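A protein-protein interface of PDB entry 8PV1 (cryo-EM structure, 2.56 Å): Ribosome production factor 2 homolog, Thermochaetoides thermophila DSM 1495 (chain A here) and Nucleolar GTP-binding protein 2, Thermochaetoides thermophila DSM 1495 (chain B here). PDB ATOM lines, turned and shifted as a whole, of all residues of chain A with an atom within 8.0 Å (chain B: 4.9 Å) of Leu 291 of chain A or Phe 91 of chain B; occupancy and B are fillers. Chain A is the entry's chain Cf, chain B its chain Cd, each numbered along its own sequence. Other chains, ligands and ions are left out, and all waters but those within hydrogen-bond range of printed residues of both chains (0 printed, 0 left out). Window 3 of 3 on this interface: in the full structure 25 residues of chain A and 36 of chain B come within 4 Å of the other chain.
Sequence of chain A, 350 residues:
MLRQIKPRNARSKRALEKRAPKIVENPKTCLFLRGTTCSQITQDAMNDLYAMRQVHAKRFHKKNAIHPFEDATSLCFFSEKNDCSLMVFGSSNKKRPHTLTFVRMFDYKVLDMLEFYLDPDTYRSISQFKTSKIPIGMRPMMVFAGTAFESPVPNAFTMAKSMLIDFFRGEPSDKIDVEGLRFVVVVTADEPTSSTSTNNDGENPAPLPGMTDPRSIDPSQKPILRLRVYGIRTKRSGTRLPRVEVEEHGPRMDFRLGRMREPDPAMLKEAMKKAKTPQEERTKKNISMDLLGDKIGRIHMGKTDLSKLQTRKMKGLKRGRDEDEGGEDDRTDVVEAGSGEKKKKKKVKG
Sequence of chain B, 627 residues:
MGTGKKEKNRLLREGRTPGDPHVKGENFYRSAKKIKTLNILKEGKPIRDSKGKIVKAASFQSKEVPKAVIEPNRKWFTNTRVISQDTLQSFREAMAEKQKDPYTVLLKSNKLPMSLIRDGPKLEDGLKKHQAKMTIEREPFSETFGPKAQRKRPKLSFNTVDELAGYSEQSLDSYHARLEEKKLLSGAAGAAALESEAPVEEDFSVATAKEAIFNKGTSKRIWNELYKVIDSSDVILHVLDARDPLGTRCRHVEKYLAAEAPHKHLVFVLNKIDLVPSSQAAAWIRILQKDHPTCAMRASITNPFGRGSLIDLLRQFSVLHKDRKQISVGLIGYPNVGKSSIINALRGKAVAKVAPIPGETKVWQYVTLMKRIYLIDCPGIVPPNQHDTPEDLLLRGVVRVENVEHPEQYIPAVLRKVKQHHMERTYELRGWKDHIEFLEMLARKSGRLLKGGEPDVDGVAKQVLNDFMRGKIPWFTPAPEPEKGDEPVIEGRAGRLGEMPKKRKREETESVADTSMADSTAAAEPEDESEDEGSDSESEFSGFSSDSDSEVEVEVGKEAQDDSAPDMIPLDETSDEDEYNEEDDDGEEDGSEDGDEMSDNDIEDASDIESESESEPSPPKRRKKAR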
ATOM      1  N   SER A 288     -26.567  24.167  -3.926  1.00  0.00           N
ATOM      2  CA  SER A 288     -25.318  23.448  -3.742  1.00  0.00           C
ATOM      3  C   SER A 288     -24.344  23.846  -4.840  1.00  0.00           C
ATOM      4  O   SER A 288     -24.693  24.542  -5.792  1.00  0.00           O
ATOM      5  CB  SER A 288     -25.542  21.932  -3.727  1.00  0.00           C
ATOM      6  OG  SER A 288     -25.928  21.457  -5.003  1.00  0.00           O
ATOM      7  N   MET A 289     -23.106  23.406  -4.674  1.00  0.00           N
ATOM      8  CA  MET A 289     -22.041  23.571  -5.649  1.00  0.00           C
ATOM      9  C   MET A 289     -21.670  22.211  -6.221  1.00  0.00           C
ATOM     10  O   MET A 289     -21.430  21.266  -5.464  1.00  0.00           O
ATOM     11  CB  MET A 289     -20.830  24.221  -4.986  1.00  0.00           C
ATOM     12  CG  MET A 289     -19.670  24.505  -5.886  1.00  0.00           C
ATOM     13  SD  MET A 289     -18.402  25.340  -4.933  1.00  0.00           S
ATOM     14  CE  MET A 289     -17.132  25.431  -6.170  1.00  0.00           C
ATOM     15  N   ASP A 290     -21.616  22.111  -7.549  1.00  0.00           N
ATOM     16  CA  ASP A 290     -21.277  20.829  -8.151  1.00  0.00           C
ATOM     17  C   ASP A 290     -19.758  20.646  -8.171  1.00  0.00           C
ATOM     18  O   ASP A 290     -18.999  21.439  -7.609  1.00  0.00           O
ATOM     19  CB  ASP A 290     -21.904  20.704  -9.542  1.00  0.00           C
ATOM     20  CG  ASP A 290     -21.143  21.462 -10.622  1.00  0.00           C
ATOM     21  OD1 ASP A 290     -20.528  22.505 -10.329  1.00  0.00           O
ATOM     22  OD2 ASP A 290     -21.166  21.006 -11.783  1.00  0.00           O
ATOM     23  N   LEU A 291     -19.301  19.584  -8.835  1.00  0.00           N
ATOM     24  CA  LEU A 291     -17.870  19.318  -8.876  1.00  0.00           C
ATOM     25  C   LEU A 291     -17.143  20.203  -9.879  1.00  0.00           C
ATOM     26  O   LEU A 291     -15.913  20.298  -9.821  1.00  0.00           O
ATOM     27  CB  LEU A 291     -17.621  17.843  -9.189  1.00  0.00           C
ATOM     28  CG  LEU A 291     -17.395  16.935  -7.979  1.00  0.00           C
ATOM     29  CD1 LEU A 291     -16.899  15.566  -8.417  1.00  0.00           C
ATOM     30  CD2 LEU A 291     -16.424  17.566  -6.991  1.00  0.00           C
ATOM     31  N   LEU A 292     -17.865  20.850 -10.793  1.00  0.00           N
ATOM     32  CA  LEU A 292     -17.277  21.806 -11.720  1.00  0.00           C
ATOM     33  C   LEU A 292     -17.393  23.245 -11.239  1.00  0.00           C
ATOM     34  O   LEU A 292     -16.818  24.142 -11.861  1.00  0.00           O
ATOM     35  CB  LEU A 292     -17.922  21.678 -13.098  1.00  0.00           C
ATOM     36  CG  LEU A 292     -17.400  20.597 -14.039  1.00  0.00           C
ATOM     37  CD1 LEU A 292     -18.283  20.559 -15.263  1.00  0.00           C
ATOM     38  CD2 LEU A 292     -15.957  20.862 -14.428  1.00  0.00           C
ATOM     39  N   GLY A 293     -18.113  23.486 -10.149  1.00  0.00           N
ATOM     40  CA  GLY A 293     -18.288  24.828  -9.638  1.00  0.00           C
ATOM     41  C   GLY A 293     -19.590  25.502 -10.003  1.00  0.00           C
ATOM     42  O   GLY A 293     -19.801  26.653  -9.607  1.00  0.00           O
ATOM     43  N   ASP A 294     -20.466  24.833 -10.747  1.00  0.00           N
ATOM     44  CA  ASP A 294     -21.776  25.379 -11.063  1.00  0.00           C
ATOM     45  C   ASP A 294     -22.669  25.379  -9.830  1.00  0.00           C
ATOM     46  O   ASP A 294     -22.635  24.456  -9.008  1.00  0.00           O
ATOM     47  CB  ASP A 294     -22.441  24.567 -12.173  1.00  0.00           C
ATOM     48  CG  ASP A 294     -21.664  24.603 -13.469  1.00  0.00           C
ATOM     49  OD1 ASP A 294     -20.831  25.514 -13.638  1.00  0.00           O
ATOM     50  OD2 ASP A 294     -21.884  23.716 -14.320  1.00  0.00           O
ATOM     51  N   ILE A 296     -26.095  24.738  -8.276  1.00  0.00           N
ATOM     52  CA  ILE A 296     -27.117  23.760  -8.617  1.00  0.00           C
ATOM     53  C   ILE A 296     -28.273  23.898  -7.641  1.00  0.00           C
ATOM     54  O   ILE A 296     -28.070  23.949  -6.422  1.00  0.00           O
ATOM     55  CB  ILE A 296     -26.546  22.326  -8.593  1.00  0.00           C
ATOM     56  CG1 ILE A 296     -25.330  22.218  -9.513  1.00  0.00           C
ATOM     57  CG2 ILE A 296     -27.599  21.321  -8.998  1.00  0.00           C
ATOM     58  CD1 ILE A 296     -25.626  22.533 -10.958  1.00  0.00           C
ATOM     59  N   ILE B  83      -5.140  29.275 -14.648  1.00  0.00           N
ATOM     60  CA  ILE B  83      -5.552  28.007 -14.058  1.00  0.00           C
ATOM     61  C   ILE B  83      -4.330  27.102 -13.972  1.00  0.00           C
ATOM     62  O   ILE B  83      -3.421  27.182 -14.805  1.00  0.00           O
ATOM     63  CB  ILE B  83      -6.710  27.361 -14.860  1.00  0.00           C
ATOM     64  CG1 ILE B  83      -7.345  26.208 -14.083  1.00  0.00           C
ATOM     65  CG2 ILE B  83      -6.261  26.908 -16.245  1.00  0.00           C
ATOM     66  CD1 ILE B  83      -8.645  25.724 -14.666  1.00  0.00           C
ATOM     67  N   THR B  87      -5.710  21.855 -10.939  1.00  0.00           N
ATOM     68  CA  THR B  87      -7.106  22.264 -11.039  1.00  0.00           C
ATOM     69  C   THR B  87      -7.734  21.757 -12.332  1.00  0.00           C
ATOM     70  O   THR B  87      -8.890  21.305 -12.338  1.00  0.00           O
ATOM     71  CB  THR B  87      -7.201  23.787 -10.944  1.00  0.00           C
ATOM     72  OG1 THR B  87      -6.547  24.229  -9.749  1.00  0.00           O
ATOM     73  CG2 THR B  87      -8.644  24.239 -10.904  1.00  0.00           C
ATOM     74  N   LEU B  88      -6.976  21.804 -13.432  1.00  0.00           N
ATOM     75  CA  LEU B  88      -7.464  21.276 -14.702  1.00  0.00           C
ATOM     76  C   LEU B  88      -7.730  19.778 -14.621  1.00  0.00           C
ATOM     77  O   LEU B  88      -8.759  19.299 -15.108  1.00  0.00           O
ATOM     78  CB  LEU B  88      -6.463  21.576 -15.815  1.00  0.00           C
ATOM     79  CG  LEU B  88      -6.582  22.930 -16.509  1.00  0.00           C
ATOM     80  CD1 LEU B  88      -5.377  23.179 -17.394  1.00  0.00           C
ATOM     81  CD2 LEU B  88      -7.863  22.993 -17.316  1.00  0.00           C
ATOM     82  N   GLN B  89      -6.818  19.026 -13.997  1.00  0.00           N
ATOM     83  CA  GLN B  89      -7.003  17.584 -13.858  1.00  0.00           C
ATOM     84  C   GLN B  89      -8.194  17.261 -12.964  1.00  0.00           C
ATOM     85  O   GLN B  89      -8.940  16.307 -13.227  1.00  0.00           O
ATOM     86  CB  GLN B  89      -5.727  16.946 -13.310  1.00  0.00           C
ATOM     87  CG  GLN B  89      -5.681  15.433 -13.430  1.00  0.00           C
ATOM     88  CD  GLN B  89      -5.999  14.948 -14.831  1.00  0.00           C
ATOM     89  OE1 GLN B  89      -5.283  15.252 -15.783  1.00  0.00           O
ATOM     90  NE2 GLN B  89      -7.077  14.185 -14.962  1.00  0.00           N
ATOM     91  N   SER B  90      -8.391  18.053 -11.906  1.00  0.00           N
ATOM     92  CA  SER B  90      -9.549  17.868 -11.035  1.00  0.00           C
ATOM     93  C   SER B  90     -10.851  18.109 -11.787  1.00  0.00           C
ATOM     94  O   SER B  90     -11.825  17.368 -11.617  1.00  0.00           O
ATOM     95  CB  SER B  90      -9.445  18.800  -9.828  1.00  0.00           C
ATOM     96  OG  SER B  90      -8.239  18.585  -9.120  1.00  0.00           O
ATOM     97  N   PHE B  91     -10.884  19.135 -12.639  1.00  0.00           N
ATOM     98  CA  PHE B  91     -12.099  19.410 -13.402  1.00  0.00           C
ATOM     99  C   PHE B  91     -12.342  18.354 -14.480  1.00  0.00           C
ATOM    100  O   PHE B  91     -13.496  18.016 -14.785  1.00  0.00           O
ATOM    101  CB  PHE B  91     -12.023  20.809 -14.008  1.00  0.00           C
ATOM    102  CG  PHE B  91     -12.337  21.906 -13.034  1.00  0.00           C
ATOM    103  CD1 PHE B  91     -13.285  21.719 -12.042  1.00  0.00           C
ATOM    104  CD2 PHE B  91     -11.685  23.124 -13.106  1.00  0.00           C
ATOM    105  CE1 PHE B  91     -13.579  22.726 -11.145  1.00  0.00           C
ATOM    106  CE2 PHE B  91     -11.976  24.133 -12.211  1.00  0.00           C
ATOM    107  CZ  PHE B  91     -12.924  23.933 -11.230  1.00  0.00           C
ATOM    108  N   ARG B  92     -11.266  17.814 -15.064  1.00  0.00           N
ATOM    109  CA  ARG B  92     -11.414  16.708 -16.008  1.00  0.00           C
ATOM    110  C   ARG B  92     -11.989  15.473 -15.325  1.00  0.00           C
ATOM    111  O   ARG B  92     -12.875  14.807 -15.876  1.00  0.00           O
ATOM    112  CB  ARG B  92     -10.071  16.377 -16.658  1.00  0.00           C
ATOM    113  CG  ARG B  92      -9.543  17.450 -17.586  1.00  0.00           C
ATOM    114  CD  ARG B  92      -8.380  16.937 -18.406  1.00  0.00           C
ATOM    115  NE  ARG B  92      -7.631  18.022 -19.025  1.00  0.00           N
ATOM    116  CZ  ARG B  92      -6.441  18.436 -18.617  1.00  0.00           C
ATOM    117  NH1 ARG B  92      -5.829  17.871 -17.589  1.00  0.00           N
ATOM    118  NH2 ARG B  92      -5.847  19.439 -19.256  1.00  0.00           N
ATOM    119  N   GLU B  93     -11.512  15.164 -14.116  1.00  0.00           N
ATOM    120  CA  GLU B  93     -12.090  14.060 -13.353  1.00  0.00           C
ATOM    121  C   GLU B  93     -13.539  14.349 -12.969  1.00  0.00           C
ATOM    122  O   GLU B  93     -14.367  13.431 -12.901  1.00  0.00           O
ATOM    123  CB  GLU B  93     -11.250  13.791 -12.107  1.00  0.00           C
ATOM    124  CG  GLU B  93     -10.123  12.803 -12.332  1.00  0.00           C
ATOM    125  CD  GLU B  93      -8.970  13.008 -11.373  1.00  0.00           C
ATOM    126  OE1 GLU B  93      -7.837  12.604 -11.708  1.00  0.00           O
ATOM    127  OE2 GLU B  93      -9.195  13.571 -10.281  1.00  0.00           O
ATOM    128  N   ALA B  94     -13.858  15.621 -12.711  1.00  0.00           N
ATOM    129  CA  ALA B  94     -15.233  16.004 -12.404  1.00  0.00           C
ATOM    130  C   ALA B  94     -16.170  15.719 -13.572  1.00  0.00           C
ATOM    131  O   ALA B  94     -17.265  15.173 -13.380  1.00  0.00           O
ATOM    132  CB  ALA B  94     -15.287  17.483 -12.027  1.00  0.00           C
ATOM    133  N   MET B  95     -15.757  16.070 -14.792  1.00  0.00           N
ATOM    134  CA  MET B  95     -16.598  15.755 -15.946  1.00  0.00           C
ATOM    135  C   MET B  95     -16.591  14.263 -16.252  1.00  0.00           C
ATOM    136  O   MET B  95     -17.531  13.743 -16.864  1.00  0.00           O
ATOM    137  CB  MET B  95     -16.183  16.539 -17.187  1.00  0.00           C
ATOM    138  CG  MET B  95     -16.407  18.015 -17.096  1.00  0.00           C
ATOM    139  SD  MET B  95     -15.820  18.820 -18.585  1.00  0.00           S
ATOM    140  CE  MET B  95     -17.060  18.244 -19.739  1.00  0.00           C
ATOM    141  N   GLU B  97     -16.733  11.988 -13.873  1.00  0.00           N
ATOM    142  CA  GLU B  97     -17.709  11.442 -12.936  1.00  0.00           C
ATOM    143  C   GLU B  97     -19.053  12.161 -12.958  1.00  0.00           C
ATOM    144  O   GLU B  97     -19.884  11.885 -12.089  1.00  0.00           O
ATOM    145  CB  GLU B  97     -17.156  11.463 -11.507  1.00  0.00           C
ATOM    146  CG  GLU B  97     -15.744  10.932 -11.367  1.00  0.00           C
ATOM    147  CD  GLU B  97     -15.108  11.328 -10.052  1.00  0.00           C
ATOM    148  OE1 GLU B  97     -15.843  11.786  -9.154  1.00  0.00           O
ATOM    149  OE2 GLU B  97     -13.877  11.175  -9.914  1.00  0.00           O
ATOM    150  N   ASN B 110     -20.221  28.106 -14.159  1.00  0.00           N
ATOM    151  CA  ASN B 110     -18.883  28.480 -13.729  1.00  0.00           C
ATOM    152  C   ASN B 110     -18.055  28.821 -14.960  1.00  0.00           C
ATOM    153  O   ASN B 110     -17.981  28.027 -15.902  1.00  0.00           O
ATOM    154  CB  ASN B 110     -18.235  27.347 -12.934  1.00  0.00           C
ATOM    155  CG  ASN B 110     -17.032  27.806 -12.144  1.00  0.00           C
ATOM    156  OD1 ASN B 110     -16.824  29.001 -11.949  1.00  0.00           O
ATOM    157  ND2 ASN B 110     -16.228  26.855 -11.686  1.00  0.00           N
ATOM    158  N   LEU B 112     -15.175  28.716 -17.034  1.00  0.00           N
ATOM    159  CA  LEU B 112     -14.082  27.761 -17.085  1.00  0.00           C
ATOM    160  C   LEU B 112     -13.572  27.650 -18.511  1.00  0.00           C
ATOM    161  O   LEU B 112     -14.329  27.856 -19.465  1.00  0.00           O
ATOM    162  CB  LEU B 112     -14.531  26.382 -16.581  1.00  0.00           C
ATOM    163  CG  LEU B 112     -14.642  26.229 -15.066  1.00  0.00           C
ATOM    164  CD1 LEU B 112     -15.060  24.817 -14.698  1.00  0.00           C
ATOM    165  CD2 LEU B 112     -13.324  26.598 -14.414  1.00  0.00           C
ATOM    166  N   ILE B 117     -10.933  21.194 -20.722  1.00  0.00           N
ATOM    167  CA  ILE B 117     -11.513  20.299 -19.733  1.00  0.00           C
ATOM    168  C   ILE B 117     -12.386  19.230 -20.377  1.00  0.00           C
ATOM    169  O   ILE B 117     -12.385  18.074 -19.936  1.00  0.00           O
ATOM    170  CB  ILE B 117     -12.311  21.089 -18.675  1.00  0.00           C
ATOM    171  CG1 ILE B 117     -11.464  22.230 -18.116  1.00  0.00           C
ATOM    172  CG2 ILE B 117     -12.698  20.198 -17.529  1.00  0.00           C
ATOM    173  CD1 ILE B 117     -12.236  23.200 -17.255  1.00  0.00           C
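Printed residues of chain B within 4 Å of Leu 291 of chain A: Phe 91 (3.6 Å), Ala 94 (3.6 Å) and Glu 97 (3.99 Å). Of the printed residues of chain B, Leu 292 of chain A touches Phe 91 (3.6 Å), Met 95 (3.7 Å), Asn 110 (2.8 Å) and Leu 112 (3.4 Å). Phe 91 of chain B touches just these residues of chain A: Leu 291 and Leu 292. Of the printed residues of chain A, Met 95 of chain B touches Leu 292. Printed residues of chain A within 4 Å of Glu 97 of chain B: Leu 291 (3.99 Å). The nearest printed residue of chain A that does not touch Ala 94 of chain B is Leu 292 of chain A (4.2 Å).
The side-chain carboxylate (OD1) of Asp 290 of chain A is in hydrogen-bond range of the backbone NH (N) of Gly 293 of chain A. The side-chain carboxylate of Asp 290 of chain A is in hydrogen-bond range of the backbone NH of Leu 292 of chain A (3.2 Å).
Among the printed residues, merely in contact across the chains: Leu 291 of chain A with Phe 91 of chain B (3.6 Å), Leu 291 of chain A with Ala 94 of chain B (3.6 Å), Leu 291 of chain A with Glu 97 of chain B (3.99 Å), Leu 292 of chain A with Phe 91 of chain B (3.6 Å), Leu 292 of chain A with Met 95 of chain B (3.7 Å), Leu 292 of chain A with Leu 112 of chain B (3.4 Å) and Gly 293 of chain A with Asn 110 of chain B (3.5 Å).
Of the 8 printed residues of chain A, 4 touch a printed residue of chain B. Hydrophobic or aromatic side chains of chain B that line the printed part of chain A: Phe 91, Ala 94, Met 95 and Leu 112. Among the printed residues, 9 pairs touch across the chains. Among the printed residues, no Asp or Glu carboxylate lies within 4 Å of a Lys or Arg side-chain nitrogen of the other chain.
The side-chain carboxylate of Asp 294 of chain A lies within hydrogen-bond range of the backbone NH of Asn 110 of chain B (2.7 Å). The side-chain amide nitrogen (ND2) of Asn 110 of chain B lies within hydrogen-bond range of the backbone carbonyl oxygen (O) of Leu 292 of chain A.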
